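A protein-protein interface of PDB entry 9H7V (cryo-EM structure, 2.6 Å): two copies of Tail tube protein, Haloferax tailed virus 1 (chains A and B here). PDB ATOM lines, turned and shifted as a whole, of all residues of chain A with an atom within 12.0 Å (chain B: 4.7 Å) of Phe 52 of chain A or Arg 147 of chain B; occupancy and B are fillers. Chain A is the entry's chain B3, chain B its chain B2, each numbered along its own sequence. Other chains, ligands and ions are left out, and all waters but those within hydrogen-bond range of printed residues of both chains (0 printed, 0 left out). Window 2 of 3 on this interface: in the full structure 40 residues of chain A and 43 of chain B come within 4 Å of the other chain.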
ATOM      1  N   HIS A  42       9.109 -17.769  15.557  1.00  0.00           N
ATOM      2  CA  HIS A  42       9.956 -17.868  16.734  1.00  0.00           C
ATOM      3  C   HIS A  42       9.872 -19.274  17.316  1.00  0.00           C
ATOM      4  O   HIS A  42       8.784 -19.755  17.629  1.00  0.00           O
ATOM      5  CB  HIS A  42       9.574 -16.798  17.767  1.00  0.00           C
ATOM      6  CG  HIS A  42      10.154 -15.451  17.492  1.00  0.00           C
ATOM      7  ND1 HIS A  42      10.185 -14.456  18.448  1.00  0.00           N
ATOM      8  CD2 HIS A  42      10.734 -14.934  16.389  1.00  0.00           C
ATOM      9  CE1 HIS A  42      10.753 -13.382  17.941  1.00  0.00           C
ATOM     10  NE2 HIS A  42      11.098 -13.648  16.679  1.00  0.00           N
ATOM     11  N   ALA A  43      11.037 -19.921  17.437  1.00  0.00           N
ATOM     12  CA  ALA A  43      11.167 -21.148  18.203  1.00  0.00           C
ATOM     13  C   ALA A  43      11.706 -20.805  19.588  1.00  0.00           C
ATOM     14  O   ALA A  43      12.840 -20.346  19.719  1.00  0.00           O
ATOM     15  CB  ALA A  43      12.060 -22.124  17.478  1.00  0.00           C
ATOM     16  N   GLU A  44      10.863 -21.015  20.608  1.00  0.00           N
ATOM     17  CA  GLU A  44      11.239 -20.825  21.999  1.00  0.00           C
ATOM     18  C   GLU A  44      11.700 -22.166  22.562  1.00  0.00           C
ATOM     19  O   GLU A  44      10.945 -23.137  22.556  1.00  0.00           O
ATOM     20  CB  GLU A  44      10.074 -20.245  22.804  1.00  0.00           C
ATOM     21  CG  GLU A  44       9.751 -18.801  22.459  1.00  0.00           C
ATOM     22  CD  GLU A  44       8.689 -18.161  23.338  1.00  0.00           C
ATOM     23  OE1 GLU A  44       7.511 -18.558  23.228  1.00  0.00           O
ATOM     24  OE2 GLU A  44       9.044 -17.275  24.136  1.00  0.00           O
ATOM     25  N   LEU A  45      12.949 -22.197  23.042  1.00  0.00           N
ATOM     26  CA  LEU A  45      13.612 -23.432  23.430  1.00  0.00           C
ATOM     27  C   LEU A  45      13.948 -23.399  24.920  1.00  0.00           C
ATOM     28  O   LEU A  45      14.341 -22.359  25.445  1.00  0.00           O
ATOM     29  CB  LEU A  45      14.860 -23.626  22.559  1.00  0.00           C
ATOM     30  CG  LEU A  45      14.619 -23.725  21.049  1.00  0.00           C
ATOM     31  CD1 LEU A  45      15.928 -23.649  20.283  1.00  0.00           C
ATOM     32  CD2 LEU A  45      13.862 -24.996  20.684  1.00  0.00           C
ATOM     33  N   TYR A  46      13.792 -24.556  25.580  1.00  0.00           N
ATOM     34  CA  TYR A  46      13.866 -24.688  27.030  1.00  0.00           C
ATOM     35  C   TYR A  46      14.898 -25.755  27.407  1.00  0.00           C
ATOM     36  O   TYR A  46      15.147 -26.667  26.623  1.00  0.00           O
ATOM     37  CB  TYR A  46      12.472 -25.014  27.577  1.00  0.00           C
ATOM     38  CG  TYR A  46      11.461 -23.894  27.499  1.00  0.00           C
ATOM     39  CD1 TYR A  46      10.719 -23.662  26.348  1.00  0.00           C
ATOM     40  CD2 TYR A  46      11.228 -23.072  28.592  1.00  0.00           C
ATOM     41  CE1 TYR A  46       9.789 -22.633  26.279  1.00  0.00           C
ATOM     42  CE2 TYR A  46      10.301 -22.040  28.541  1.00  0.00           C
ATOM     43  CZ  TYR A  46       9.579 -21.819  27.380  1.00  0.00           C
ATOM     44  OH  TYR A  46       8.665 -20.807  27.323  1.00  0.00           O
ATOM     45  N   THR A  47      15.501 -25.635  28.604  1.00  0.00           N
ATOM     46  CA  THR A  47      16.482 -26.601  29.093  1.00  0.00           C
ATOM     47  C   THR A  47      15.801 -27.679  29.935  1.00  0.00           C
ATOM     48  O   THR A  47      14.587 -27.647  30.126  1.00  0.00           O
ATOM     49  CB  THR A  47      17.625 -25.972  29.909  1.00  0.00           C
ATOM     50  OG1 THR A  47      17.153 -25.546  31.189  1.00  0.00           O
ATOM     51  CG2 THR A  47      18.338 -24.838  29.212  1.00  0.00           C
ATOM     52  N   ILE A  48      16.615 -28.598  30.474  1.00  0.00           N
ATOM     53  CA  ILE A  48      16.132 -29.839  31.062  1.00  0.00           C
ATOM     54  C   ILE A  48      15.750 -29.667  32.536  1.00  0.00           C
ATOM     55  O   ILE A  48      14.946 -30.446  33.046  1.00  0.00           O
ATOM     56  CB  ILE A  48      17.125 -30.996  30.816  1.00  0.00           C
ATOM     57  CG1 ILE A  48      16.454 -32.358  31.003  1.00  0.00           C
ATOM     58  CG2 ILE A  48      18.394 -30.854  31.652  1.00  0.00           C
ATOM     59  CD1 ILE A  48      17.103 -33.454  30.222  1.00  0.00           C
ATOM     60  N   ASP A  49      16.301 -28.651  33.214  1.00  0.00           N
ATOM     61  CA  ASP A  49      16.130 -28.527  34.655  1.00  0.00           C
ATOM     62  C   ASP A  49      15.615 -27.133  35.025  1.00  0.00           C
ATOM     63  O   ASP A  49      15.938 -26.608  36.090  1.00  0.00           O
ATOM     64  CB  ASP A  49      17.417 -28.920  35.393  1.00  0.00           C
ATOM     65  CG  ASP A  49      17.280 -29.043  36.904  1.00  0.00           C
ATOM     66  OD1 ASP A  49      16.175 -29.381  37.375  1.00  0.00           O
ATOM     67  OD2 ASP A  49      18.282 -28.789  37.601  1.00  0.00           O
ATOM     68  N   SER A  50      14.789 -26.550  34.148  1.00  0.00           N
ATOM     69  CA  SER A  50      14.323 -25.183  34.326  1.00  0.00           C
ATOM     70  C   SER A  50      12.984 -24.976  33.630  1.00  0.00           C
ATOM     71  O   SER A  50      12.729 -25.573  32.589  1.00  0.00           O
ATOM     72  CB  SER A  50      15.349 -24.202  33.811  1.00  0.00           C
ATOM     73  OG  SER A  50      14.871 -22.867  33.898  1.00  0.00           O
ATOM     74  N   THR A  51      12.161 -24.089  34.208  1.00  0.00           N
ATOM     75  CA  THR A  51      10.907 -23.646  33.617  1.00  0.00           C
ATOM     76  C   THR A  51      11.149 -22.452  32.694  1.00  0.00           C
ATOM     77  O   THR A  51      10.268 -22.083  31.919  1.00  0.00           O
ATOM     78  CB  THR A  51       9.854 -23.314  34.686  1.00  0.00           C
ATOM     79  OG1 THR A  51      10.326 -22.221  35.475  1.00  0.00           O
ATOM     80  CG2 THR A  51       9.508 -24.486  35.578  1.00  0.00           C
ATOM     81  N   PHE A  52      12.349 -21.861  32.782  1.00  0.00           N
ATOM     82  CA  PHE A  52      12.694 -20.654  32.047  1.00  0.00           C
ATOM     83  C   PHE A  52      13.259 -21.015  30.674  1.00  0.00           C
ATOM     84  O   PHE A  52      13.826 -22.092  30.489  1.00  0.00           O
ATOM     85  CB  PHE A  52      13.682 -19.801  32.848  1.00  0.00           C
ATOM     86  CG  PHE A  52      13.146 -19.046  34.043  1.00  0.00           C
ATOM     87  CD1 PHE A  52      11.841 -19.202  34.496  1.00  0.00           C
ATOM     88  CD2 PHE A  52      13.982 -18.190  34.747  1.00  0.00           C
ATOM     89  CE1 PHE A  52      11.382 -18.504  35.606  1.00  0.00           C
ATOM     90  CE2 PHE A  52      13.526 -17.495  35.859  1.00  0.00           C
ATOM     91  CZ  PHE A  52      12.226 -17.652  36.286  1.00  0.00           C
ATOM     92  N   ARG A  53      13.098 -20.079  29.731  1.00  0.00           N
ATOM     93  CA  ARG A  53      13.511 -20.194  28.341  1.00  0.00           C
ATOM     94  C   ARG A  53      15.033 -20.117  28.254  1.00  0.00           C
ATOM     95  O   ARG A  53      15.647 -19.257  28.885  1.00  0.00           O
ATOM     96  CB  ARG A  53      12.860 -19.045  27.564  1.00  0.00           C
ATOM     97  CG  ARG A  53      12.767 -19.231  26.057  1.00  0.00           C
ATOM     98  CD  ARG A  53      11.995 -18.077  25.438  1.00  0.00           C
ATOM     99  NE  ARG A  53      12.680 -16.794  25.570  1.00  0.00           N
ATOM    100  CZ  ARG A  53      12.137 -15.594  25.374  1.00  0.00           C
ATOM    101  NH1 ARG A  53      12.879 -14.512  25.527  1.00  0.00           N
ATOM    102  NH2 ARG A  53      10.868 -15.470  25.027  1.00  0.00           N
ATOM    103  N   ASP A  54      15.628 -21.024  27.468  1.00  0.00           N
ATOM    104  CA  ASP A  54      17.063 -21.024  27.229  1.00  0.00           C
ATOM    105  C   ASP A  54      17.392 -20.029  26.122  1.00  0.00           C
ATOM    106  O   ASP A  54      18.186 -19.110  26.325  1.00  0.00           O
ATOM    107  CB  ASP A  54      17.588 -22.419  26.874  1.00  0.00           C
ATOM    108  CG  ASP A  54      19.093 -22.573  27.046  1.00  0.00           C
ATOM    109  OD1 ASP A  54      19.670 -21.861  27.897  1.00  0.00           O
ATOM    110  OD2 ASP A  54      19.676 -23.419  26.344  1.00  0.00           O
ATOM    111  N   GLU A  55      16.768 -20.239  24.956  1.00  0.00           N
ATOM    112  CA  GLU A  55      17.045 -19.494  23.740  1.00  0.00           C
ATOM    113  C   GLU A  55      15.745 -19.271  22.975  1.00  0.00           C
ATOM    114  O   GLU A  55      14.774 -20.001  23.168  1.00  0.00           O
ATOM    115  CB  GLU A  55      18.014 -20.272  22.844  1.00  0.00           C
ATOM    116  CG  GLU A  55      19.418 -20.429  23.412  1.00  0.00           C
ATOM    117  CD  GLU A  55      20.302 -19.193  23.470  1.00  0.00           C
ATOM    118  OE1 GLU A  55      19.829 -18.087  23.128  1.00  0.00           O
ATOM    119  OE2 GLU A  55      21.478 -19.339  23.856  1.00  0.00           O
ATOM    120  N   VAL A  56      15.748 -18.255  22.106  1.00  0.00           N
ATOM    121  CA  VAL A  56      14.681 -18.043  21.139  1.00  0.00           C
ATOM    122  C   VAL A  56      15.313 -17.706  19.789  1.00  0.00           C
ATOM    123  O   VAL A  56      16.273 -16.938  19.731  1.00  0.00           O
ATOM    124  CB  VAL A  56      13.644 -17.007  21.628  1.00  0.00           C
ATOM    125  CG1 VAL A  56      14.256 -15.666  22.010  1.00  0.00           C
ATOM    126  CG2 VAL A  56      12.480 -16.825  20.664  1.00  0.00           C
ATOM    127  N   LYS A  57      14.785 -18.315  18.716  1.00  0.00           N
ATOM    128  CA  LYS A  57      15.404 -18.248  17.399  1.00  0.00           C
ATOM    129  C   LYS A  57      14.381 -17.904  16.318  1.00  0.00           C
ATOM    130  O   LYS A  57      13.239 -18.355  16.367  1.00  0.00           O
ATOM    131  CB  LYS A  57      16.121 -19.563  17.065  1.00  0.00           C
ATOM    132  CG  LYS A  57      17.426 -19.824  17.812  1.00  0.00           C
ATOM    133  CD  LYS A  57      18.564 -18.905  17.415  1.00  0.00           C
ATOM    134  CE  LYS A  57      19.864 -19.208  18.126  1.00  0.00           C
ATOM    135  NZ  LYS A  57      20.991 -18.423  17.567  1.00  0.00           N
ATOM    136  N   TYR B  40       2.509 -19.453  33.034  1.00  0.00           N
ATOM    137  CA  TYR B  40       3.095 -20.780  33.031  1.00  0.00           C
ATOM    138  C   TYR B  40       2.065 -21.759  32.476  1.00  0.00           C
ATOM    139  O   TYR B  40       0.864 -21.578  32.677  1.00  0.00           O
ATOM    140  CB  TYR B  40       3.414 -21.241  34.457  1.00  0.00           C
ATOM    141  CG  TYR B  40       4.484 -20.503  35.226  1.00  0.00           C
ATOM    142  CD1 TYR B  40       4.195 -19.341  35.928  1.00  0.00           C
ATOM    143  CD2 TYR B  40       5.770 -21.017  35.334  1.00  0.00           C
ATOM    144  CE1 TYR B  40       5.164 -18.684  36.675  1.00  0.00           C
ATOM    145  CE2 TYR B  40       6.749 -20.375  36.078  1.00  0.00           C
ATOM    146  CZ  TYR B  40       6.447 -19.202  36.750  1.00  0.00           C
ATOM    147  OH  TYR B  40       7.405 -18.560  37.479  1.00  0.00           O
ATOM    148  N   HIS B  61       7.561 -21.268  31.393  1.00  0.00           N
ATOM    149  CA  HIS B  61       7.358 -19.868  31.721  1.00  0.00           C
ATOM    150  C   HIS B  61       7.598 -18.988  30.499  1.00  0.00           C
ATOM    151  O   HIS B  61       8.535 -19.221  29.734  1.00  0.00           O
ATOM    152  CB  HIS B  61       8.225 -19.459  32.918  1.00  0.00           C
ATOM    153  CG  HIS B  61       7.943 -18.086  33.432  1.00  0.00           C
ATOM    154  ND1 HIS B  61       6.678 -17.681  33.812  1.00  0.00           N
ATOM    155  CD2 HIS B  61       8.757 -17.032  33.648  1.00  0.00           C
ATOM    156  CE1 HIS B  61       6.724 -16.432  34.227  1.00  0.00           C
ATOM    157  NE2 HIS B  61       7.988 -16.013  34.135  1.00  0.00           N
ATOM    158  N   ASN B  62       6.723 -17.989  30.336  1.00  0.00           N
ATOM    159  CA  ASN B  62       6.955 -16.839  29.476  1.00  0.00           C
ATOM    160  C   ASN B  62       6.127 -15.663  29.987  1.00  0.00           C
ATOM    161  O   ASN B  62       5.181 -15.849  30.751  1.00  0.00           O
ATOM    162  CB  ASN B  62       6.714 -17.142  27.991  1.00  0.00           C
ATOM    163  CG  ASN B  62       5.252 -17.224  27.603  1.00  0.00           C
ATOM    164  OD1 ASN B  62       4.747 -16.359  26.891  1.00  0.00           O
ATOM    165  ND2 ASN B  62       4.565 -18.260  28.057  1.00  0.00           N
ATOM    166  N   VAL B  63       6.512 -14.455  29.564  1.00  0.00           N
ATOM    167  CA  VAL B  63       5.730 -13.258  29.813  1.00  0.00           C
ATOM    168  C   VAL B  63       5.163 -12.794  28.475  1.00  0.00           C
ATOM    169  O   VAL B  63       5.918 -12.464  27.566  1.00  0.00           O
ATOM    170  CB  VAL B  63       6.563 -12.152  30.494  1.00  0.00           C
ATOM    171  CG1 VAL B  63       5.727 -10.921  30.806  1.00  0.00           C
ATOM    172  CG2 VAL B  63       7.254 -12.650  31.754  1.00  0.00           C
ATOM    173  N   GLU B 120      12.477  -9.197  31.104  1.00  0.00           N
ATOM    174  CA  GLU B 120      13.729  -9.443  30.402  1.00  0.00           C
ATOM    175  C   GLU B 120      13.475 -10.166  29.081  1.00  0.00           C
ATOM    176  O   GLU B 120      12.579 -11.005  28.987  1.00  0.00           O
ATOM    177  CB  GLU B 120      14.727 -10.214  31.272  1.00  0.00           C
ATOM    178  CG  GLU B 120      14.243 -11.588  31.715  1.00  0.00           C
ATOM    179  CD  GLU B 120      15.313 -12.581  32.142  1.00  0.00           C
ATOM    180  OE1 GLU B 120      16.504 -12.208  32.177  1.00  0.00           O
ATOM    181  OE2 GLU B 120      14.949 -13.734  32.441  1.00  0.00           O
ATOM    182  N   ASN B 121      14.286  -9.809  28.074  1.00  0.00           N
ATOM    183  CA  ASN B 121      14.432 -10.514  26.807  1.00  0.00           C
ATOM    184  C   ASN B 121      13.089 -10.660  26.088  1.00  0.00           C
ATOM    185  O   ASN B 121      12.703 -11.765  25.710  1.00  0.00           O
ATOM    186  CB  ASN B 121      15.182 -11.844  26.967  1.00  0.00           C
ATOM    187  CG  ASN B 121      16.589 -11.709  27.516  1.00  0.00           C
ATOM    188  OD1 ASN B 121      17.165 -10.622  27.531  1.00  0.00           O
ATOM    189  ND2 ASN B 121      17.156 -12.817  27.963  1.00  0.00           N
ATOM    190  N   SER B 145       7.080 -12.211  23.524  1.00  0.00           N
ATOM    191  CA  SER B 145       7.280 -12.975  24.746  1.00  0.00           C
ATOM    192  C   SER B 145       8.614 -12.638  25.409  1.00  0.00           C
ATOM    193  O   SER B 145       9.664 -12.681  24.771  1.00  0.00           O
ATOM    194  CB  SER B 145       7.124 -14.457  24.509  1.00  0.00           C
ATOM    195  OG  SER B 145       8.039 -14.912  23.524  1.00  0.00           O
ATOM    196  N   GLY B 146       8.534 -12.298  26.702  1.00  0.00           N
ATOM    197  CA  GLY B 146       9.688 -12.144  27.571  1.00  0.00           C
ATOM    198  C   GLY B 146      10.012 -13.446  28.298  1.00  0.00           C
ATOM    199  O   GLY B 146       9.161 -14.329  28.403  1.00  0.00           O
ATOM    200  N   ARG B 147      11.251 -13.545  28.793  1.00  0.00           N
ATOM    201  CA  ARG B 147      11.737 -14.733  29.476  1.00  0.00           C
ATOM    202  C   ARG B 147      11.168 -14.793  30.894  1.00  0.00           C
ATOM    203  O   ARG B 147      10.678 -15.843  31.306  1.00  0.00           O
ATOM    204  CB  ARG B 147      13.269 -14.785  29.453  1.00  0.00           C
ATOM    205  CG  ARG B 147      13.871 -15.999  30.145  1.00  0.00           C
ATOM    206  CD  ARG B 147      15.381 -16.005  30.024  1.00  0.00           C
ATOM    207  NE  ARG B 147      15.997 -17.144  30.692  1.00  0.00           N
ATOM    208  CZ  ARG B 147      16.436 -17.160  31.949  1.00  0.00           C
ATOM    209  NH1 ARG B 147      16.979 -18.260  32.438  1.00  0.00           N
ATOM    210  NH2 ARG B 147      16.334 -16.087  32.714  1.00  0.00           N
ATOM    211  N   SER B 148      11.242 -13.669  31.624  1.00  0.00           N
ATOM    212  CA  SER B 148      10.791 -13.603  33.008  1.00  0.00           C
ATOM    213  C   SER B 148      10.513 -12.162  33.434  1.00  0.00           C
ATOM    214  O   SER B 148      10.922 -11.216  32.762  1.00  0.00           O
ATOM    215  CB  SER B 148      11.779 -14.274  33.938  1.00  0.00           C
ATOM    216  OG  SER B 148      12.940 -13.479  34.122  1.00  0.00           O
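Hydrophobic or aromatic side chains of chain A within 4 Å of the printed part of chain B: Tyr 46 and Phe 52. Along chain B the printed residues that touch a printed residue of chain A span positions 61 to 147. Among the printed residues, no Asp or Glu carboxylate lies within 4 Å of a Lys or Arg side-chain nitrogen of the other chain.
His 61 of chain B touches Phe 52 of chain A (CD2 to CE1, 3.6 Å). CB of Phe 52 of chain A touches NH1 of Arg 147 of chain B, at 3.7 Å. NH2 of Arg 53 of chain A touches C of Gly 146 of chain B (3.9 Å).
O of Val 63 of chain B is in hydrogen-bond range of N of Gly 146 of chain B (2.8 Å). The side-chain carboxylate of Glu 120 of chain B lies within salt-bridge range of the guanidinium group of Arg 147 of chain B. The side-chain carboxylate of Glu 44 of chain A is in salt-bridge range of the guanidinium group of Arg 53 of chain A, at 2.7 Å. The side-chain hydroxyl (OG) of Ser 50 of chain A sits at hydrogen-bond distance from the backbone NH (N) of Phe 52 of chain A (2.9 Å).
O of His 61 of chain B sits at hydrogen-bond distance from OH of Tyr 46 of chain A (2.9 Å). The backbone NH of His 61 of chain B lies within hydrogen-bond range of the backbone carbonyl oxygen of Thr 51 of chain A (2.9 Å). The backbone carbonyl oxygen (O) of Asn 121 of chain B lies within hydrogen-bond range of the guanidinium group (NH1) of Arg 53 of chain A (2.8 Å). The side-chain carboxylate (OE2) of Glu 44 of chain A lies within hydrogen-bond range of the side-chain hydroxyl (OG) of Ser 145 of chain B (2.6 Å). O of Ser 145 of chain B lies within hydrogen-bond range of NH2 of Arg 53 of chain A. The guanidinium group (NE) of Arg 147 of chain B lies within hydrogen-bond range of the backbone carbonyl oxygen (O) of Arg 53 of chain A.
No position is printed for both chains.
Printed residues of chain B within 4 Å of Glu 44 of chain A: Ser 145. Leu 45 of chain A touches none of the printed residues of chain B. Of the printed residues of chain B, Tyr 46 of chain A touches His 61. Ser 50 of chain A touches none of the printed residues of chain B. Of the printed residues of chain B, Thr 51 of chain A touches His 61. Printed residues of chain B within 4 Å of Phe 52 of chain A: His 61 (3.6 Å) and Arg 147 (3.7 Å). Printed residues of chain B within 4 Å of Arg 53 of chain A: Asn 121, Ser 145, Gly 146 and Arg 147. No residue of chain A comes within 4 Å of Asn 62 of chain B. No residue of chain A comes within 4 Å of Val 63 of chain B. No residue of chain A comes within 4 Å of Glu 120 of chain B. Asn 121 of chain B touches just one residue of chain A: Arg 53 (2.8 Å). Of chain A, only Glu 44 and Arg 53 come within 4 Å of Ser 145 of chain B. Of chain A, only Arg 53 comes within 4 Å of Gly 146 of chain B. No residue of chain A comes within 4 Å of Ser 148 of chain B. The nearest residue of chain B that does not touch Phe 52 of chain A is Ser 148 of chain B (4.1 Å). The nearest residue of chain A that does not touch Arg 147 of chain B is Asp 54 of chain A (5.1 Å). The nearest printed residue of chain B that does not touch Arg 53 of chain A is His 61 of chain B (4.6 Å).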
